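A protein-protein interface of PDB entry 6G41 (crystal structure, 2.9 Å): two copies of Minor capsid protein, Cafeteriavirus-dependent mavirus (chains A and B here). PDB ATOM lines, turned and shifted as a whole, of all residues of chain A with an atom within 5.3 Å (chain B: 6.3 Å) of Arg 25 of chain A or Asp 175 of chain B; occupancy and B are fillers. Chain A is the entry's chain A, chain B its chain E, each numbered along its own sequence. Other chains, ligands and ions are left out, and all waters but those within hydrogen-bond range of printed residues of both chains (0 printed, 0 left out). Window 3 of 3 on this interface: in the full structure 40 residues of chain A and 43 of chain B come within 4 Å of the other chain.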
ATOM      1  N   GLY A  23      16.052 -38.196   7.665  1.00  0.00           N
ATOM      2  CA  GLY A  23      15.269 -37.142   6.988  1.00  0.00           C
ATOM      3  C   GLY A  23      15.785 -35.744   7.314  1.00  0.00           C
ATOM      4  O   GLY A  23      16.599 -35.587   8.222  1.00  0.00           O
ATOM      5  N   PRO A  24      15.324 -34.712   6.578  1.00  0.00           N
ATOM      6  CA  PRO A  24      15.742 -33.348   6.922  1.00  0.00           C
ATOM      7  C   PRO A  24      15.289 -32.964   8.332  1.00  0.00           C
ATOM      8  O   PRO A  24      14.113 -33.153   8.666  1.00  0.00           O
ATOM      9  CB  PRO A  24      15.042 -32.480   5.866  1.00  0.00           C
ATOM     10  CG  PRO A  24      14.753 -33.404   4.736  1.00  0.00           C
ATOM     11  CD  PRO A  24      14.489 -34.738   5.364  1.00  0.00           C
ATOM     12  N   ARG A  25      16.232 -32.471   9.145  1.00  0.00           N
ATOM     13  CA  ARG A  25      16.001 -32.162  10.571  1.00  0.00           C
ATOM     14  C   ARG A  25      15.426 -33.331  11.418  1.00  0.00           C
ATOM     15  O   ARG A  25      14.801 -33.108  12.459  1.00  0.00           O
ATOM     16  CB  ARG A  25      15.099 -30.924  10.707  1.00  0.00           C
ATOM     17  CG  ARG A  25      15.690 -29.635  10.150  1.00  0.00           C
ATOM     18  CD  ARG A  25      15.591 -28.511  11.177  1.00  0.00           C
ATOM     19  NE  ARG A  25      15.981 -27.202  10.650  1.00  0.00           N
ATOM     20  CZ  ARG A  25      15.202 -26.392   9.931  1.00  0.00           C
ATOM     21  NH1 ARG A  25      13.957 -26.743   9.602  1.00  0.00           N
ATOM     22  NH2 ARG A  25      15.680 -25.217   9.522  1.00  0.00           N
ATOM     23  N   GLY A  26      15.654 -34.563  10.976  1.00  0.00           N
ATOM     24  CA  GLY A  26      15.034 -35.739  11.581  1.00  0.00           C
ATOM     25  C   GLY A  26      13.528 -35.859  11.357  1.00  0.00           C
ATOM     26  O   GLY A  26      12.818 -36.386  12.215  1.00  0.00           O
ATOM     27  N   SER A  27      13.039 -35.398  10.207  1.00  0.00           N
ATOM     28  CA  SER A  27      11.592 -35.327   9.965  1.00  0.00           C
ATOM     29  C   SER A  27      10.906 -36.684   9.774  1.00  0.00           C
ATOM     30  O   SER A  27       9.691 -36.787   9.988  1.00  0.00           O
ATOM     31  CB  SER A  27      11.272 -34.416   8.785  1.00  0.00           C
ATOM     32  OG  SER A  27      11.854 -34.900   7.599  1.00  0.00           O
ATOM     33  N   TYR A 248      19.484 -29.221  21.646  1.00  0.00           N
ATOM     34  CA  TYR A 248      20.260 -30.320  21.096  1.00  0.00           C
ATOM     35  C   TYR A 248      21.310 -30.743  22.109  1.00  0.00           C
ATOM     36  O   TYR A 248      21.941 -29.900  22.753  1.00  0.00           O
ATOM     37  CB  TYR A 248      20.930 -29.879  19.798  1.00  0.00           C
ATOM     38  CG  TYR A 248      19.964 -29.673  18.653  1.00  0.00           C
ATOM     39  CD1 TYR A 248      19.597 -30.730  17.832  1.00  0.00           C
ATOM     40  CD2 TYR A 248      19.422 -28.428  18.379  1.00  0.00           C
ATOM     41  CE1 TYR A 248      18.715 -30.551  16.775  1.00  0.00           C
ATOM     42  CE2 TYR A 248      18.538 -28.245  17.323  1.00  0.00           C
ATOM     43  CZ  TYR A 248      18.187 -29.312  16.524  1.00  0.00           C
ATOM     44  OH  TYR A 248      17.313 -29.159  15.468  1.00  0.00           O
ATOM     45  N   LEU A 292      18.692 -37.848  14.281  1.00  0.00           N
ATOM     46  CA  LEU A 292      18.944 -36.712  13.412  1.00  0.00           C
ATOM     47  C   LEU A 292      19.929 -37.209  12.365  1.00  0.00           C
ATOM     48  O   LEU A 292      20.546 -38.266  12.554  1.00  0.00           O
ATOM     49  CB  LEU A 292      19.550 -35.544  14.189  1.00  0.00           C
ATOM     50  CG  LEU A 292      18.723 -34.963  15.340  1.00  0.00           C
ATOM     51  CD1 LEU A 292      19.545 -33.948  16.107  1.00  0.00           C
ATOM     52  CD2 LEU A 292      17.440 -34.320  14.853  1.00  0.00           C
ATOM     53  N   PRO A 293      20.094 -36.464  11.254  1.00  0.00           N
ATOM     54  CA  PRO A 293      21.145 -36.805  10.277  1.00  0.00           C
ATOM     55  C   PRO A 293      22.560 -36.873  10.851  1.00  0.00           C
ATOM     56  O   PRO A 293      23.370 -37.659  10.373  1.00  0.00           O
ATOM     57  CB  PRO A 293      21.060 -35.662   9.269  1.00  0.00           C
ATOM     58  CG  PRO A 293      19.638 -35.234   9.329  1.00  0.00           C
ATOM     59  CD  PRO A 293      19.251 -35.357  10.773  1.00  0.00           C
ATOM     60  N   ILE B  85      16.247 -15.388  -0.683  1.00  0.00           N
ATOM     61  CA  ILE B  85      17.642 -15.737  -0.432  1.00  0.00           C
ATOM     62  C   ILE B  85      18.522 -15.050  -1.464  1.00  0.00           C
ATOM     63  O   ILE B  85      18.303 -15.186  -2.663  1.00  0.00           O
ATOM     64  CB  ILE B  85      17.843 -17.266  -0.487  1.00  0.00           C
ATOM     65  CG1 ILE B  85      17.036 -17.932   0.630  1.00  0.00           C
ATOM     66  CG2 ILE B  85      19.314 -17.642  -0.348  1.00  0.00           C
ATOM     67  CD1 ILE B  85      16.727 -19.379   0.370  1.00  0.00           C
ATOM     68  N   MET B 157      22.013 -16.918   7.393  1.00  0.00           N
ATOM     69  CA  MET B 157      21.402 -18.247   7.305  1.00  0.00           C
ATOM     70  C   MET B 157      22.393 -19.332   7.621  1.00  0.00           C
ATOM     71  O   MET B 157      23.506 -19.318   7.110  1.00  0.00           O
ATOM     72  CB  MET B 157      20.900 -18.517   5.895  1.00  0.00           C
ATOM     73  CG  MET B 157      19.696 -17.661   5.535  1.00  0.00           C
ATOM     74  SD  MET B 157      19.519 -17.605   3.573  1.00  0.00           S
ATOM     75  CE  MET B 157      19.209 -19.527   3.268  1.00  0.00           C
ATOM     76  N   PHE B 158      21.993 -20.274   8.470  1.00  0.00           N
ATOM     77  CA  PHE B 158      22.750 -21.505   8.736  1.00  0.00           C
ATOM     78  C   PHE B 158      21.978 -22.691   8.143  1.00  0.00           C
ATOM     79  O   PHE B 158      20.739 -22.709   8.189  1.00  0.00           O
ATOM     80  CB  PHE B 158      22.890 -21.729  10.251  1.00  0.00           C
ATOM     81  CG  PHE B 158      23.998 -20.946  10.922  1.00  0.00           C
ATOM     82  CD1 PHE B 158      24.549 -19.794  10.364  1.00  0.00           C
ATOM     83  CD2 PHE B 158      24.454 -21.353  12.169  1.00  0.00           C
ATOM     84  CE1 PHE B 158      25.548 -19.095  11.022  1.00  0.00           C
ATOM     85  CE2 PHE B 158      25.454 -20.659  12.828  1.00  0.00           C
ATOM     86  CZ  PHE B 158      25.999 -19.528  12.257  1.00  0.00           C
ATOM     87  N   ASP B 160      21.318 -27.090   8.070  1.00  0.00           N
ATOM     88  CA  ASP B 160      20.998 -28.045   9.138  1.00  0.00           C
ATOM     89  C   ASP B 160      22.219 -28.519   9.947  1.00  0.00           C
ATOM     90  O   ASP B 160      22.126 -28.688  11.164  1.00  0.00           O
ATOM     91  CB  ASP B 160      20.233 -29.252   8.572  1.00  0.00           C
ATOM     92  CG  ASP B 160      19.590 -30.117   9.662  1.00  0.00           C
ATOM     93  OD1 ASP B 160      19.125 -29.557  10.680  1.00  0.00           O
ATOM     94  OD2 ASP B 160      19.537 -31.358   9.490  1.00  0.00           O
ATOM     95  N   ARG B 163      23.341 -25.455  12.084  1.00  0.00           N
ATOM     96  CA  ARG B 163      22.302 -25.354  13.107  1.00  0.00           C
ATOM     97  C   ARG B 163      22.556 -26.257  14.313  1.00  0.00           C
ATOM     98  O   ARG B 163      22.431 -25.809  15.446  1.00  0.00           O
ATOM     99  CB  ARG B 163      20.950 -25.705  12.469  1.00  0.00           C
ATOM    100  CG  ARG B 163      19.758 -25.787  13.410  1.00  0.00           C
ATOM    101  CD  ARG B 163      19.327 -24.419  13.877  1.00  0.00           C
ATOM    102  NE  ARG B 163      18.040 -24.505  14.558  1.00  0.00           N
ATOM    103  CZ  ARG B 163      17.860 -24.748  15.856  1.00  0.00           C
ATOM    104  NH1 ARG B 163      16.617 -24.793  16.330  1.00  0.00           N
ATOM    105  NH2 ARG B 163      18.889 -24.936  16.683  1.00  0.00           N
ATOM    106  N   ASP B 172      15.316 -19.079  13.997  1.00  0.00           N
ATOM    107  CA  ASP B 172      13.979 -19.190  13.419  1.00  0.00           C
ATOM    108  C   ASP B 172      14.112 -20.080  12.183  1.00  0.00           C
ATOM    109  O   ASP B 172      14.945 -19.812  11.316  1.00  0.00           O
ATOM    110  CB  ASP B 172      13.454 -17.801  13.037  1.00  0.00           C
ATOM    111  CG  ASP B 172      12.057 -17.833  12.415  1.00  0.00           C
ATOM    112  OD1 ASP B 172      11.292 -18.791  12.654  1.00  0.00           O
ATOM    113  OD2 ASP B 172      11.717 -16.876  11.687  1.00  0.00           O
ATOM    114  N   ASP B 173      13.299 -21.130  12.107  1.00  0.00           N
ATOM    115  CA  ASP B 173      13.357 -22.080  10.993  1.00  0.00           C
ATOM    116  C   ASP B 173      12.462 -21.622   9.840  1.00  0.00           C
ATOM    117  O   ASP B 173      11.241 -21.555  10.003  1.00  0.00           O
ATOM    118  CB  ASP B 173      12.936 -23.477  11.459  1.00  0.00           C
ATOM    119  CG  ASP B 173      13.760 -23.986  12.654  1.00  0.00           C
ATOM    120  OD1 ASP B 173      14.957 -23.626  12.801  1.00  0.00           O
ATOM    121  OD2 ASP B 173      13.197 -24.764  13.454  1.00  0.00           O
ATOM    122  N   ILE B 174      13.068 -21.312   8.687  1.00  0.00           N
ATOM    123  CA  ILE B 174      12.317 -20.925   7.473  1.00  0.00           C
ATOM    124  C   ILE B 174      11.908 -22.111   6.588  1.00  0.00           C
ATOM    125  O   ILE B 174      10.767 -22.170   6.128  1.00  0.00           O
ATOM    126  CB  ILE B 174      13.042 -19.845   6.614  1.00  0.00           C
ATOM    127  CG1 ILE B 174      14.457 -20.273   6.155  1.00  0.00           C
ATOM    128  CG2 ILE B 174      13.092 -18.532   7.383  1.00  0.00           C
ATOM    129  CD1 ILE B 174      14.975 -19.522   4.940  1.00  0.00           C
ATOM    130  N   ASP B 175      12.833 -23.044   6.371  1.00  0.00           N
ATOM    131  CA  ASP B 175      12.678 -24.138   5.402  1.00  0.00           C
ATOM    132  C   ASP B 175      12.956 -25.463   6.086  1.00  0.00           C
ATOM    133  O   ASP B 175      13.265 -25.500   7.272  1.00  0.00           O
ATOM    134  CB  ASP B 175      13.665 -23.955   4.231  1.00  0.00           C
ATOM    135  CG  ASP B 175      13.141 -23.054   3.138  1.00  0.00           C
ATOM    136  OD1 ASP B 175      11.917 -23.031   2.902  1.00  0.00           O
ATOM    137  OD2 ASP B 175      13.972 -22.383   2.488  1.00  0.00           O
ATOM    138  N   GLU B 176      12.838 -26.544   5.317  1.00  0.00           N
ATOM    139  CA  GLU B 176      13.316 -27.866   5.722  1.00  0.00           C
ATOM    140  C   GLU B 176      14.822 -27.885   6.008  1.00  0.00           C
ATOM    141  O   GLU B 176      15.269 -28.643   6.865  1.00  0.00           O
ATOM    142  CB  GLU B 176      13.014 -28.914   4.643  1.00  0.00           C
ATOM    143  CG  GLU B 176      11.535 -29.143   4.354  1.00  0.00           C
ATOM    144  CD  GLU B 176      11.261 -30.495   3.705  1.00  0.00           C
ATOM    145  OE1 GLU B 176      11.898 -30.803   2.678  1.00  0.00           O
ATOM    146  OE2 GLU B 176      10.404 -31.250   4.215  1.00  0.00           O
ATOM    147  N   GLU B 177      15.589 -27.071   5.279  1.00  0.00           N
ATOM    148  CA  GLU B 177      17.051 -27.027   5.410  1.00  0.00           C
ATOM    149  C   GLU B 177      17.553 -25.834   6.239  1.00  0.00           C
ATOM    150  O   GLU B 177      18.261 -26.024   7.237  1.00  0.00           O
ATOM    151  CB  GLU B 177      17.701 -27.028   4.012  1.00  0.00           C
ATOM    152  CG  GLU B 177      19.225 -27.183   3.981  1.00  0.00           C
ATOM    153  CD  GLU B 177      19.745 -28.493   4.571  1.00  0.00           C
ATOM    154  OE1 GLU B 177      19.006 -29.502   4.593  1.00  0.00           O
ATOM    155  OE2 GLU B 177      20.914 -28.516   5.013  1.00  0.00           O
ATOM    156  N   TYR B 178      17.178 -24.621   5.832  1.00  0.00           N
ATOM    157  CA  TYR B 178      17.811 -23.388   6.347  1.00  0.00           C
ATOM    158  C   TYR B 178      17.116 -22.748   7.546  1.00  0.00           C
ATOM    159  O   TYR B 178      15.909 -22.876   7.716  1.00  0.00           O
ATOM    160  CB  TYR B 178      18.000 -22.385   5.205  1.00  0.00           C
ATOM    161  CG  TYR B 178      18.912 -22.978   4.169  1.00  0.00           C
ATOM    162  CD1 TYR B 178      20.291 -23.020   4.379  1.00  0.00           C
ATOM    163  CD2 TYR B 178      18.401 -23.584   3.020  1.00  0.00           C
ATOM    164  CE1 TYR B 178      21.142 -23.606   3.453  1.00  0.00           C
ATOM    165  CE2 TYR B 178      19.243 -24.174   2.084  1.00  0.00           C
ATOM    166  CZ  TYR B 178      20.613 -24.183   2.307  1.00  0.00           C
ATOM    167  OH  TYR B 178      21.464 -24.766   1.403  1.00  0.00           O
ATOM    168  N   SER B 179      17.921 -22.084   8.377  1.00  0.00           N
ATOM    169  CA  SER B 179      17.456 -21.371   9.565  1.00  0.00           C
ATOM    170  C   SER B 179      18.089 -19.983   9.604  1.00  0.00           C
ATOM    171  O   SER B 179      19.249 -19.816   9.237  1.00  0.00           O
ATOM    172  CB  SER B 179      17.830 -22.128  10.843  1.00  0.00           C
ATOM    173  OG  SER B 179      17.156 -23.367  10.933  1.00  0.00           O
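Of chain B, only Asp 160 (3.5 Å), Asp 173 (3.7 Å), Asp 175 (2.7 Å), Glu 176 (3.5 Å), Glu 177 (3.5 Å), Tyr 178 (3.0 Å) and Ser 179 (2.8 Å) come within 4 Å of Arg 25 of chain A.
Of chain A, only Arg 25 (2.7 Å) comes within 4 Å of Asp 175 of chain B.
Printed residues of chain A within 4 Å of Glu 177 of chain B: Arg 25.
Of the printed residues of chain A, Ser 179 of chain B touches Arg 25.
Printed residues of chain B within 4 Å of Tyr 248 of chain A: Arg 163 (3.4 Å).
Printed residues of chain B within 4 Å of Pro 24 of chain A: Glu 176.
Gly 23 of chain A touches none of the printed residues of chain B.
The nearest printed residue of chain A that does not touch Glu 177 of chain B is Pro 24 of chain A (5.1 Å).
No position is printed for both chains.
Of the 10 pairs that touch across the chains among the printed residues, none has its exchanged pair printed and touching as well.
OG of Ser 27 of chain A lies within hydrogen-bond range of O of Pro 24 of chain A (3.0 Å).
The backbone NH (N) of Phe 158 of chain B is in hydrogen-bond range of the backbone carbonyl oxygen (O) of Ser 179 of chain B (2.9 Å).
N of Asp 160 of chain B sits at hydrogen-bond distance from O of Glu 177 of chain B, at 3.3 Å.
The guanidinium group of Arg 163 of chain B lies within salt-bridge range of the side-chain carboxylate of Asp 173 of chain B, at 3.7 Å.
OD1 of Asp 173 of chain B sits at hydrogen-bond distance from OG of Ser 179 of chain B (2.9 Å).
Glu 176 of chain B touches Pro 24 of chain A.
O of Glu 176 of chain B touches CG of Arg 25 of chain A (3.5 Å).
O of Glu 177 of chain B touches NH2 of Arg 25 of chain A, 3.5 Å away.
Arg 163 of chain B touches Tyr 248 of chain A.
Asp 160 of chain B touches Pro 293 of chain A (OD2 to CG, 3.9 Å).
Printed residues of chain A that touch a printed residue of chain B: Pro 24, Arg 25, Tyr 248 and Pro 293.
Along chain A the printed residues that touch a printed residue of chain B span positions 24 to 293.
Among the printed residues, 10 pairs touch across the chains.
Among the printed residues, Asp or Glu carboxylates within 4 Å of a Lys or Arg side-chain nitrogen of the other chain: Arg 25 of chain A with Asp 160 of chain B (3.9 Å) and Arg 25 of chain A with Asp 173 of chain B (3.7 Å).
NE of Arg 25 of chain A lies within salt-bridge range of OD1 of Asp 160 of chain B (3.9 Å).
The side-chain carboxylate of Asp 173 of chain B is in salt-bridge range of the guanidinium group of Arg 25 of chain A (3.7 Å).
The guanidinium group (NH1) of Arg 25 of chain A sits at hydrogen-bond distance from the backbone carbonyl oxygen (O) of Asp 175 of chain B (2.7 Å).
The backbone carbonyl oxygen of Tyr 178 of chain B sits at hydrogen-bond distance from the guanidinium group of Arg 25 of chain A, at 3.0 Å.
The guanidinium group (NH2) of Arg 25 of chain A lies within hydrogen-bond range of the side-chain hydroxyl (OG) of Ser 179 of chain B.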
